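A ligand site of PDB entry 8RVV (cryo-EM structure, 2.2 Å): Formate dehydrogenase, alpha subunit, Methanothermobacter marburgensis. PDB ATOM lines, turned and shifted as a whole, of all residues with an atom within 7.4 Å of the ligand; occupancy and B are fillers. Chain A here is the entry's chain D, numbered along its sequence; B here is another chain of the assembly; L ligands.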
ATOM      1  N   LEU A   6      -2.823  -3.247  30.735  1.00  0.00           N
ATOM      2  CA  LEU A   6      -2.176  -2.637  29.582  1.00  0.00           C
ATOM      3  C   LEU A   6      -0.722  -3.067  29.525  1.00  0.00           C
ATOM      4  O   LEU A   6      -0.071  -3.258  30.555  1.00  0.00           O
ATOM      5  CB  LEU A   6      -2.283  -1.116  29.680  1.00  0.00           C
ATOM      6  CG  LEU A   6      -1.453  -0.245  28.728  1.00  0.00           C
ATOM      7  CD1 LEU A   6      -2.137  -0.146  27.372  1.00  0.00           C
ATOM      8  CD2 LEU A   6      -1.245   1.124  29.328  1.00  0.00           C
ATOM      9  N   CYS A   7      -0.221  -3.230  28.306  1.00  0.00           N
ATOM     10  CA  CYS A   7       1.203  -3.490  28.125  1.00  0.00           C
ATOM     11  C   CYS A   7       1.988  -2.187  28.290  1.00  0.00           C
ATOM     12  O   CYS A   7       1.691  -1.214  27.592  1.00  0.00           O
ATOM     13  CB  CYS A   7       1.479  -4.093  26.746  1.00  0.00           C
ATOM     14  SG  CYS A   7       3.238  -4.245  26.372  1.00  0.00           S
ATOM     15  N   PRO A   8       2.978  -2.129  29.176  1.00  0.00           N
ATOM     16  CA  PRO A   8       3.720  -0.888  29.387  1.00  0.00           C
ATOM     17  C   PRO A   8       4.961  -0.727  28.529  1.00  0.00           C
ATOM     18  O   PRO A   8       5.657   0.281  28.670  1.00  0.00           O
ATOM     19  CB  PRO A   8       4.107  -1.001  30.860  1.00  0.00           C
ATOM     20  CG  PRO A   8       4.364  -2.457  31.050  1.00  0.00           C
ATOM     21  CD  PRO A   8       3.439  -3.190  30.102  1.00  0.00           C
ATOM     22  N   SER A   9       5.260  -1.672  27.634  1.00  0.00           N
ATOM     23  CA  SER A   9       6.578  -1.718  27.010  1.00  0.00           C
ATOM     24  C   SER A   9       6.760  -0.678  25.921  1.00  0.00           C
ATOM     25  O   SER A   9       7.878  -0.168  25.751  1.00  0.00           O
ATOM     26  CB  SER A   9       6.833  -3.125  26.466  1.00  0.00           C
ATOM     27  OG  SER A   9       6.896  -4.057  27.520  1.00  0.00           O
ATOM     28  N   CYS A  10       5.721  -0.332  25.168  1.00  0.00           N
ATOM     29  CA  CYS A  10       5.794   0.795  24.246  1.00  0.00           C
ATOM     30  C   CYS A  10       4.462   1.531  24.287  1.00  0.00           C
ATOM     31  O   CYS A  10       3.591   1.223  25.100  1.00  0.00           O
ATOM     32  CB  CYS A  10       6.161   0.340  22.819  1.00  0.00           C
ATOM     33  SG  CYS A  10       4.775  -0.232  21.840  1.00  0.00           S
ATOM     34  N   SER A  11       4.298   2.492  23.384  1.00  0.00           N
ATOM     35  CA  SER A  11       3.167   3.402  23.439  1.00  0.00           C
ATOM     36  C   SER A  11       1.942   2.910  22.688  1.00  0.00           C
ATOM     37  O   SER A  11       0.904   3.578  22.722  1.00  0.00           O
ATOM     38  CB  SER A  11       3.571   4.772  22.904  1.00  0.00           C
ATOM     39  OG  SER A  11       4.262   4.670  21.673  1.00  0.00           O
ATOM     40  N   ALA A  12       2.013   1.765  22.012  1.00  0.00           N
ATOM     41  CA  ALA A  12       0.807   1.134  21.524  1.00  0.00           C
ATOM     42  C   ALA A  12      -0.063   0.716  22.699  1.00  0.00           C
ATOM     43  O   ALA A  12       0.445   0.316  23.761  1.00  0.00           O
ATOM     44  CB  ALA A  12       1.155  -0.083  20.655  1.00  0.00           C
ATOM     45  N   GLY A  13      -1.369   0.828  22.541  1.00  0.00           N
ATOM     46  CA  GLY A  13      -2.260   0.556  23.652  1.00  0.00           C
ATOM     47  C   GLY A  13      -2.677  -0.893  23.791  1.00  0.00           C
ATOM     48  O   GLY A  13      -3.811  -1.174  24.166  1.00  0.00           O
ATOM     49  N   CYS A  14      -1.769  -1.824  23.508  1.00  0.00           N
ATOM     50  CA  CYS A  14      -2.126  -3.231  23.499  1.00  0.00           C
ATOM     51  C   CYS A  14      -2.552  -3.704  24.886  1.00  0.00           C
ATOM     52  O   CYS A  14      -1.925  -3.369  25.892  1.00  0.00           O
ATOM     53  CB  CYS A  14      -0.958  -4.076  22.997  1.00  0.00           C
ATOM     54  SG  CYS A  14      -0.450  -3.709  21.315  1.00  0.00           S
ATOM     55  N   GLY A  15      -3.621  -4.491  24.925  1.00  0.00           N
ATOM     56  CA  GLY A  15      -4.095  -5.097  26.159  1.00  0.00           C
ATOM     57  C   GLY A  15      -3.561  -6.503  26.318  1.00  0.00           C
ATOM     58  O   GLY A  15      -3.408  -7.240  25.345  1.00  0.00           O
ATOM     59  N   VAL A  16      -3.260  -6.878  27.567  1.00  0.00           N
ATOM     60  CA  VAL A  16      -2.773  -8.210  27.909  1.00  0.00           C
ATOM     61  C   VAL A  16      -3.533  -8.679  29.138  1.00  0.00           C
ATOM     62  O   VAL A  16      -4.213  -7.899  29.808  1.00  0.00           O
ATOM     63  CB  VAL A  16      -1.253  -8.217  28.165  1.00  0.00           C
ATOM     64  CG1 VAL A  16      -0.510  -7.677  26.968  1.00  0.00           C
ATOM     65  CG2 VAL A  16      -0.905  -7.408  29.408  1.00  0.00           C
ATOM     66  N   VAL A  36      -7.299  -2.605  20.279  1.00  0.00           N
ATOM     67  CA  VAL A  36      -6.035  -2.159  19.698  1.00  0.00           C
ATOM     68  C   VAL A  36      -5.295  -3.331  19.038  1.00  0.00           C
ATOM     69  O   VAL A  36      -4.774  -3.195  17.934  1.00  0.00           O
ATOM     70  CB  VAL A  36      -5.162  -1.484  20.776  1.00  0.00           C
ATOM     71  CG1 VAL A  36      -3.698  -1.453  20.341  1.00  0.00           C
ATOM     72  CG2 VAL A  36      -5.667  -0.081  21.048  1.00  0.00           C
ATOM     73  N   ASN A  37      -5.251  -4.475  19.707  1.00  0.00           N
ATOM     74  CA  ASN A  37      -4.456  -5.606  19.237  1.00  0.00           C
ATOM     75  C   ASN A  37      -5.208  -6.923  19.157  1.00  0.00           C
ATOM     76  O   ASN A  37      -4.662  -7.868  18.589  1.00  0.00           O
ATOM     77  CB  ASN A  37      -3.227  -5.790  20.136  1.00  0.00           C
ATOM     78  CG  ASN A  37      -3.588  -6.051  21.586  1.00  0.00           C
ATOM     79  OD1 ASN A  37      -4.483  -5.414  22.138  1.00  0.00           O
ATOM     80  ND2 ASN A  37      -2.877  -6.978  22.215  1.00  0.00           N
ATOM     81  N   LYS A  40      -3.281 -10.024  20.169  1.00  0.00           N
ATOM     82  CA  LYS A  40      -1.977 -10.233  19.566  1.00  0.00           C
ATOM     83  C   LYS A  40      -0.969  -9.328  20.269  1.00  0.00           C
ATOM     84  O   LYS A  40      -1.242  -8.151  20.507  1.00  0.00           O
ATOM     85  CB  LYS A  40      -2.008  -9.936  18.072  1.00  0.00           C
ATOM     86  CG  LYS A  40      -3.066 -10.713  17.315  1.00  0.00           C
ATOM     87  CD  LYS A  40      -3.367 -10.098  15.958  1.00  0.00           C
ATOM     88  CE  LYS A  40      -4.395 -10.907  15.196  1.00  0.00           C
ATOM     89  NZ  LYS A  40      -3.847 -12.186  14.668  1.00  0.00           N
ATOM     90  N   THR A  41       0.189  -9.877  20.605  1.00  0.00           N
ATOM     91  CA  THR A  41       1.234  -9.109  21.262  1.00  0.00           C
ATOM     92  C   THR A  41       2.582  -9.491  20.665  1.00  0.00           C
ATOM     93  O   THR A  41       2.781 -10.609  20.186  1.00  0.00           O
ATOM     94  CB  THR A  41       1.266  -9.347  22.779  1.00  0.00           C
ATOM     95  OG1 THR A  41       1.130 -10.747  23.055  1.00  0.00           O
ATOM     96  CG2 THR A  41       0.156  -8.596  23.472  1.00  0.00           C
ATOM     97  N   CYS A  42       3.507  -8.534  20.697  1.00  0.00           N
ATOM     98  CA  CYS A  42       4.899  -8.824  20.425  1.00  0.00           C
ATOM     99  C   CYS A  42       5.527  -9.466  21.662  1.00  0.00           C
ATOM    100  O   CYS A  42       4.861  -9.728  22.656  1.00  0.00           O
ATOM    101  CB  CYS A  42       5.625  -7.543  20.013  1.00  0.00           C
ATOM    102  SG  CYS A  42       5.959  -6.392  21.351  1.00  0.00           S
ATOM    103  N   ARG A  43       6.834  -9.743  21.587  1.00  0.00           N
ATOM    104  CA  ARG A  43       7.494 -10.448  22.681  1.00  0.00           C
ATOM    105  C   ARG A  43       7.416  -9.657  23.986  1.00  0.00           C
ATOM    106  O   ARG A  43       7.162 -10.237  25.057  1.00  0.00           O
ATOM    107  CB  ARG A  43       8.954 -10.719  22.320  1.00  0.00           C
ATOM    108  CG  ARG A  43       9.598 -11.846  23.095  1.00  0.00           C
ATOM    109  CD  ARG A  43       9.231 -13.199  22.510  1.00  0.00           C
ATOM    110  NE  ARG A  43       9.755 -14.310  23.296  1.00  0.00           N
ATOM    111  CZ  ARG A  43      10.981 -14.790  23.189  1.00  0.00           C
ATOM    112  NH1 ARG A  43      11.866 -14.266  22.359  1.00  0.00           N
ATOM    113  NH2 ARG A  43      11.338 -15.827  23.942  1.00  0.00           N
ATOM    114  N   ALA A  44       7.625  -8.342  23.928  1.00  0.00           N
ATOM    115  CA  ALA A  44       7.625  -7.532  25.142  1.00  0.00           C
ATOM    116  C   ALA A  44       6.270  -7.590  25.846  1.00  0.00           C
ATOM    117  O   ALA A  44       6.208  -7.595  27.080  1.00  0.00           O
ATOM    118  CB  ALA A  44       7.996  -6.092  24.811  1.00  0.00           C
ATOM    119  N   GLY A  45       5.185  -7.618  25.079  1.00  0.00           N
ATOM    120  CA  GLY A  45       3.866  -7.727  25.678  1.00  0.00           C
ATOM    121  C   GLY A  45       3.698  -9.004  26.469  1.00  0.00           C
ATOM    122  O   GLY A  45       3.054  -9.020  27.510  1.00  0.00           O
ATOM    123  N   ARG A  46       4.266 -10.106  25.968  1.00  0.00           N
ATOM    124  CA  ARG A  46       4.177 -11.371  26.682  1.00  0.00           C
ATOM    125  C   ARG A  46       5.203 -11.478  27.805  1.00  0.00           C
ATOM    126  O   ARG A  46       5.048 -12.342  28.677  1.00  0.00           O
ATOM    127  CB  ARG A  46       4.356 -12.531  25.691  1.00  0.00           C
ATOM    128  CG  ARG A  46       3.031 -13.056  25.164  1.00  0.00           C
ATOM    129  CD  ARG A  46       3.196 -13.881  23.901  1.00  0.00           C
ATOM    130  NE  ARG A  46       3.514 -13.054  22.734  1.00  0.00           N
ATOM    131  CZ  ARG A  46       4.641 -13.112  22.043  1.00  0.00           C
ATOM    132  NH1 ARG A  46       5.632 -13.923  22.377  1.00  0.00           N
ATOM    133  NH2 ARG A  46       4.781 -12.328  20.977  1.00  0.00           N
ATOM    134  N   CYS A  48       5.886  -8.729  29.780  1.00  0.00           N
ATOM    135  CA  CYS A  48       5.625  -7.655  30.746  1.00  0.00           C
ATOM    136  C   CYS A  48       5.241  -8.178  32.132  1.00  0.00           C
ATOM    137  O   CYS A  48       5.341  -7.424  33.108  1.00  0.00           O
ATOM    138  CB  CYS A  48       4.514  -6.743  30.217  1.00  0.00           C
ATOM    139  SG  CYS A  48       2.832  -7.385  30.375  1.00  0.00           S
ATOM    140  N   ILE A 149       7.408  -0.255  12.470  1.00  0.00           N
ATOM    141  CA  ILE A 149       7.103  -1.638  12.837  1.00  0.00           C
ATOM    142  C   ILE A 149       7.869  -2.038  14.086  1.00  0.00           C
ATOM    143  O   ILE A 149       7.302  -2.625  15.021  1.00  0.00           O
ATOM    144  CB  ILE A 149       7.394  -2.584  11.669  1.00  0.00           C
ATOM    145  CG1 ILE A 149       6.440  -2.328  10.501  1.00  0.00           C
ATOM    146  CG2 ILE A 149       7.282  -4.035  12.117  1.00  0.00           C
ATOM    147  CD1 ILE A 149       6.962  -2.807   9.167  1.00  0.00           C
ATOM    148  N   THR A 150       9.161  -1.736  14.128  1.00  0.00           N
ATOM    149  CA  THR A 150       9.965  -2.085  15.293  1.00  0.00           C
ATOM    150  C   THR A 150       9.563  -1.276  16.518  1.00  0.00           C
ATOM    151  O   THR A 150       9.494  -1.800  17.631  1.00  0.00           O
ATOM    152  CB  THR A 150      11.443  -1.889  14.983  1.00  0.00           C
ATOM    153  OG1 THR A 150      11.755  -2.494  13.727  1.00  0.00           O
ATOM    154  CG2 THR A 150      12.312  -2.520  16.069  1.00  0.00           C
ATOM    155  N   CYS A 151       9.289   0.021  16.328  1.00  0.00           N
ATOM    156  CA  CYS A 151       8.893   0.865  17.458  1.00  0.00           C
ATOM    157  C   CYS A 151       7.573   0.392  18.065  1.00  0.00           C
ATOM    158  O   CYS A 151       7.440   0.349  19.289  1.00  0.00           O
ATOM    159  CB  CYS A 151       8.792   2.323  17.004  1.00  0.00           C
ATOM    160  SG  CYS A 151      10.384   3.111  16.727  1.00  0.00           S
ATOM    161  N   ALA A 152       6.596   0.057  17.232  1.00  0.00           N
ATOM    162  CA  ALA A 152       5.285  -0.396  17.694  1.00  0.00           C
ATOM    163  C   ALA A 152       4.790  -1.463  16.732  1.00  0.00           C
ATOM    164  O   ALA A 152       4.120  -1.150  15.729  1.00  0.00           O
ATOM    165  CB  ALA A 152       4.308   0.769  17.797  1.00  0.00           C
ATOM    166  N   PRO A 153       5.093  -2.736  16.995  1.00  0.00           N
ATOM    167  CA  PRO A 153       4.681  -3.793  16.049  1.00  0.00           C
ATOM    168  C   PRO A 153       3.195  -3.811  15.744  1.00  0.00           C
ATOM    169  O   PRO A 153       2.810  -4.110  14.600  1.00  0.00           O
ATOM    170  CB  PRO A 153       5.128  -5.065  16.768  1.00  0.00           C
ATOM    171  CG  PRO A 153       6.308  -4.650  17.549  1.00  0.00           C
ATOM    172  CD  PRO A 153       6.058  -3.234  17.984  1.00  0.00           C
ATOM    173  N   LEU A 154       2.333  -3.496  16.710  1.00  0.00           N
ATOM    174  CA  LEU A 154       0.899  -3.581  16.482  1.00  0.00           C
ATOM    175  C   LEU A 154       0.334  -2.352  15.781  1.00  0.00           C
ATOM    176  O   LEU A 154      -0.845  -2.354  15.431  1.00  0.00           O
ATOM    177  CB  LEU A 154       0.167  -3.832  17.798  1.00  0.00           C
ATOM    178  CG  LEU A 154      -0.074  -5.300  18.183  1.00  0.00           C
ATOM    179  CD1 LEU A 154      -0.911  -6.027  17.138  1.00  0.00           C
ATOM    180  CD2 LEU A 154       1.236  -6.047  18.424  1.00  0.00           C
ATOM    181  N   ILE A 155       1.143  -1.309  15.570  1.00  0.00           N
ATOM    182  CA  ILE A 155       0.788  -0.261  14.613  1.00  0.00           C
ATOM    183  C   ILE A 155       1.340  -0.577  13.224  1.00  0.00           C
ATOM    184  O   ILE A 155       0.709  -0.254  12.213  1.00  0.00           O
ATOM    185  CB  ILE A 155       1.286   1.108  15.122  1.00  0.00           C
ATOM    186  CG1 ILE A 155       0.453   1.569  16.323  1.00  0.00           C
ATOM    187  CG2 ILE A 155       1.214   2.148  14.014  1.00  0.00           C
ATOM    188  CD1 ILE A 155       1.124   2.620  17.163  1.00  0.00           C
ATOM    189  N   PHE A 240       4.252   4.477  27.501  1.00  0.00           N
ATOM    190  CA  PHE A 240       2.887   4.020  27.275  1.00  0.00           C
ATOM    191  C   PHE A 240       1.837   5.051  27.640  1.00  0.00           C
ATOM    192  O   PHE A 240       0.671   4.860  27.283  1.00  0.00           O
ATOM    193  CB  PHE A 240       2.633   2.704  28.026  1.00  0.00           C
ATOM    194  CG  PHE A 240       2.716   2.829  29.518  1.00  0.00           C
ATOM    195  CD1 PHE A 240       3.919   2.726  30.173  1.00  0.00           C
ATOM    196  CD2 PHE A 240       1.563   3.017  30.266  1.00  0.00           C
ATOM    197  CE1 PHE A 240       3.996   2.825  31.547  1.00  0.00           C
ATOM    198  CE2 PHE A 240       1.630   3.116  31.642  1.00  0.00           C
ATOM    199  CZ  PHE A 240       2.850   3.017  32.272  1.00  0.00           C
ATOM    200  N   ILE B 281       7.867 -11.026  12.358  1.00  0.00           N
ATOM    201  CA  ILE B 281       8.698 -10.207  13.228  1.00  0.00           C
ATOM    202  C   ILE B 281       9.415 -11.046  14.282  1.00  0.00           C
ATOM    203  O   ILE B 281      10.044 -10.481  15.184  1.00  0.00           O
ATOM    204  CB  ILE B 281       7.878  -9.084  13.882  1.00  0.00           C
ATOM    205  CG1 ILE B 281       6.632  -9.649  14.582  1.00  0.00           C
ATOM    206  CG2 ILE B 281       7.463  -8.051  12.853  1.00  0.00           C
ATOM    207  CD1 ILE B 281       6.232  -8.881  15.810  1.00  0.00           C
HETATM  208 FE1  LIG L   1       1.720  -3.932  21.933  1.00  0.00          FE
HETATM  209 FE2  LIG L   1       4.267  -4.912  21.671  1.00  0.00          FE
HETATM  210 FE3  LIG L   1       3.377  -4.054  24.118  1.00  0.00          FE
HETATM  211 FE4  LIG L   1       3.874  -2.243  22.124  1.00  0.00          FE
HETATM  212  S1  LIG L   1       5.386  -3.594  23.160  1.00  0.00           S
HETATM  213  S2  LIG L   1       2.054  -2.296  23.489  1.00  0.00           S
HETATM  214  S3  LIG L   1       3.220  -3.439  20.292  1.00  0.00           S
HETATM  215  S4  LIG L   1       2.568  -5.814  22.906  1.00  0.00           S
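SG of Cys 10 is bound to FE4 of the ligand (2.2 Å). SG of Cys 7 is bound to FE3 of the ligand, at 2.3 Å. The side-chain sulfur of Cys 14 is bound to an iron atom (FE1) of the ligand. N of Cys 42 lies close to S4 of the ligand (3.6 Å). The side-chain sulfur (SG) of Cys 42 is bound to an iron atom (FE2) of the ligand (2.3 Å). The backbone NH (N) of Leu 154 sits close to a sulfur (S3) of the ligand (3.7 Å).
The side-chain sulfur (SG) of Cys 10 lies close to the backbone NH (N) of Ala 12 (3.4 Å). SG of Cys 10 sits close to O of Cys 151. The backbone carbonyl oxygen of Cys 14 sits at hydrogen-bond distance from the backbone NH of Cys 7 (3.0 Å). The side-chain sulfur (SG) of Cys 7 sits close to the backbone NH (N) of Ser 9 (3.5 Å). The side-chain sulfur (SG) of Cys 42 sits close to the backbone NH (N) of Ala 44. O of Cys 42 sits close to NH2 of Arg 46 (3.1 Å). The backbone carbonyl oxygen (O) of Gly 45 is in hydrogen-bond range of the side-chain sulfur (SG) of Cys 48, 3.3 Å away. The backbone carbonyl oxygen (O) of Thr 41 lies within hydrogen-bond range of the guanidinium group (NH2) of Arg 46.
The backbone carbonyl oxygen (O) of Ala 12 sits close to a sulfur (S2) of the ligand. Ser 9 touches the ligand. Thr 41 touches the ligand. Ala 44 touches the ligand (CB to S1, 3.97 Å). Gly 45 touches the ligand (CA to S4, 3.6 Å). CD of Pro 153 touches S3 of the ligand, at 3.7 Å. Hydrophobic or aromatic side chains that line the ligand: Ala 12, Ala 44, Pro 153 and Leu 154. 11 residues have an atom within 4 Å of the ligand: Cys 7, Ser 9, Cys 10, Ala 12, Cys 14, Thr 41, Cys 42, Ala 44, Gly 45, Pro 153 and Leu 154. The nearest printed residue that does not touch the ligand is Ala 152 (4.4 Å).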
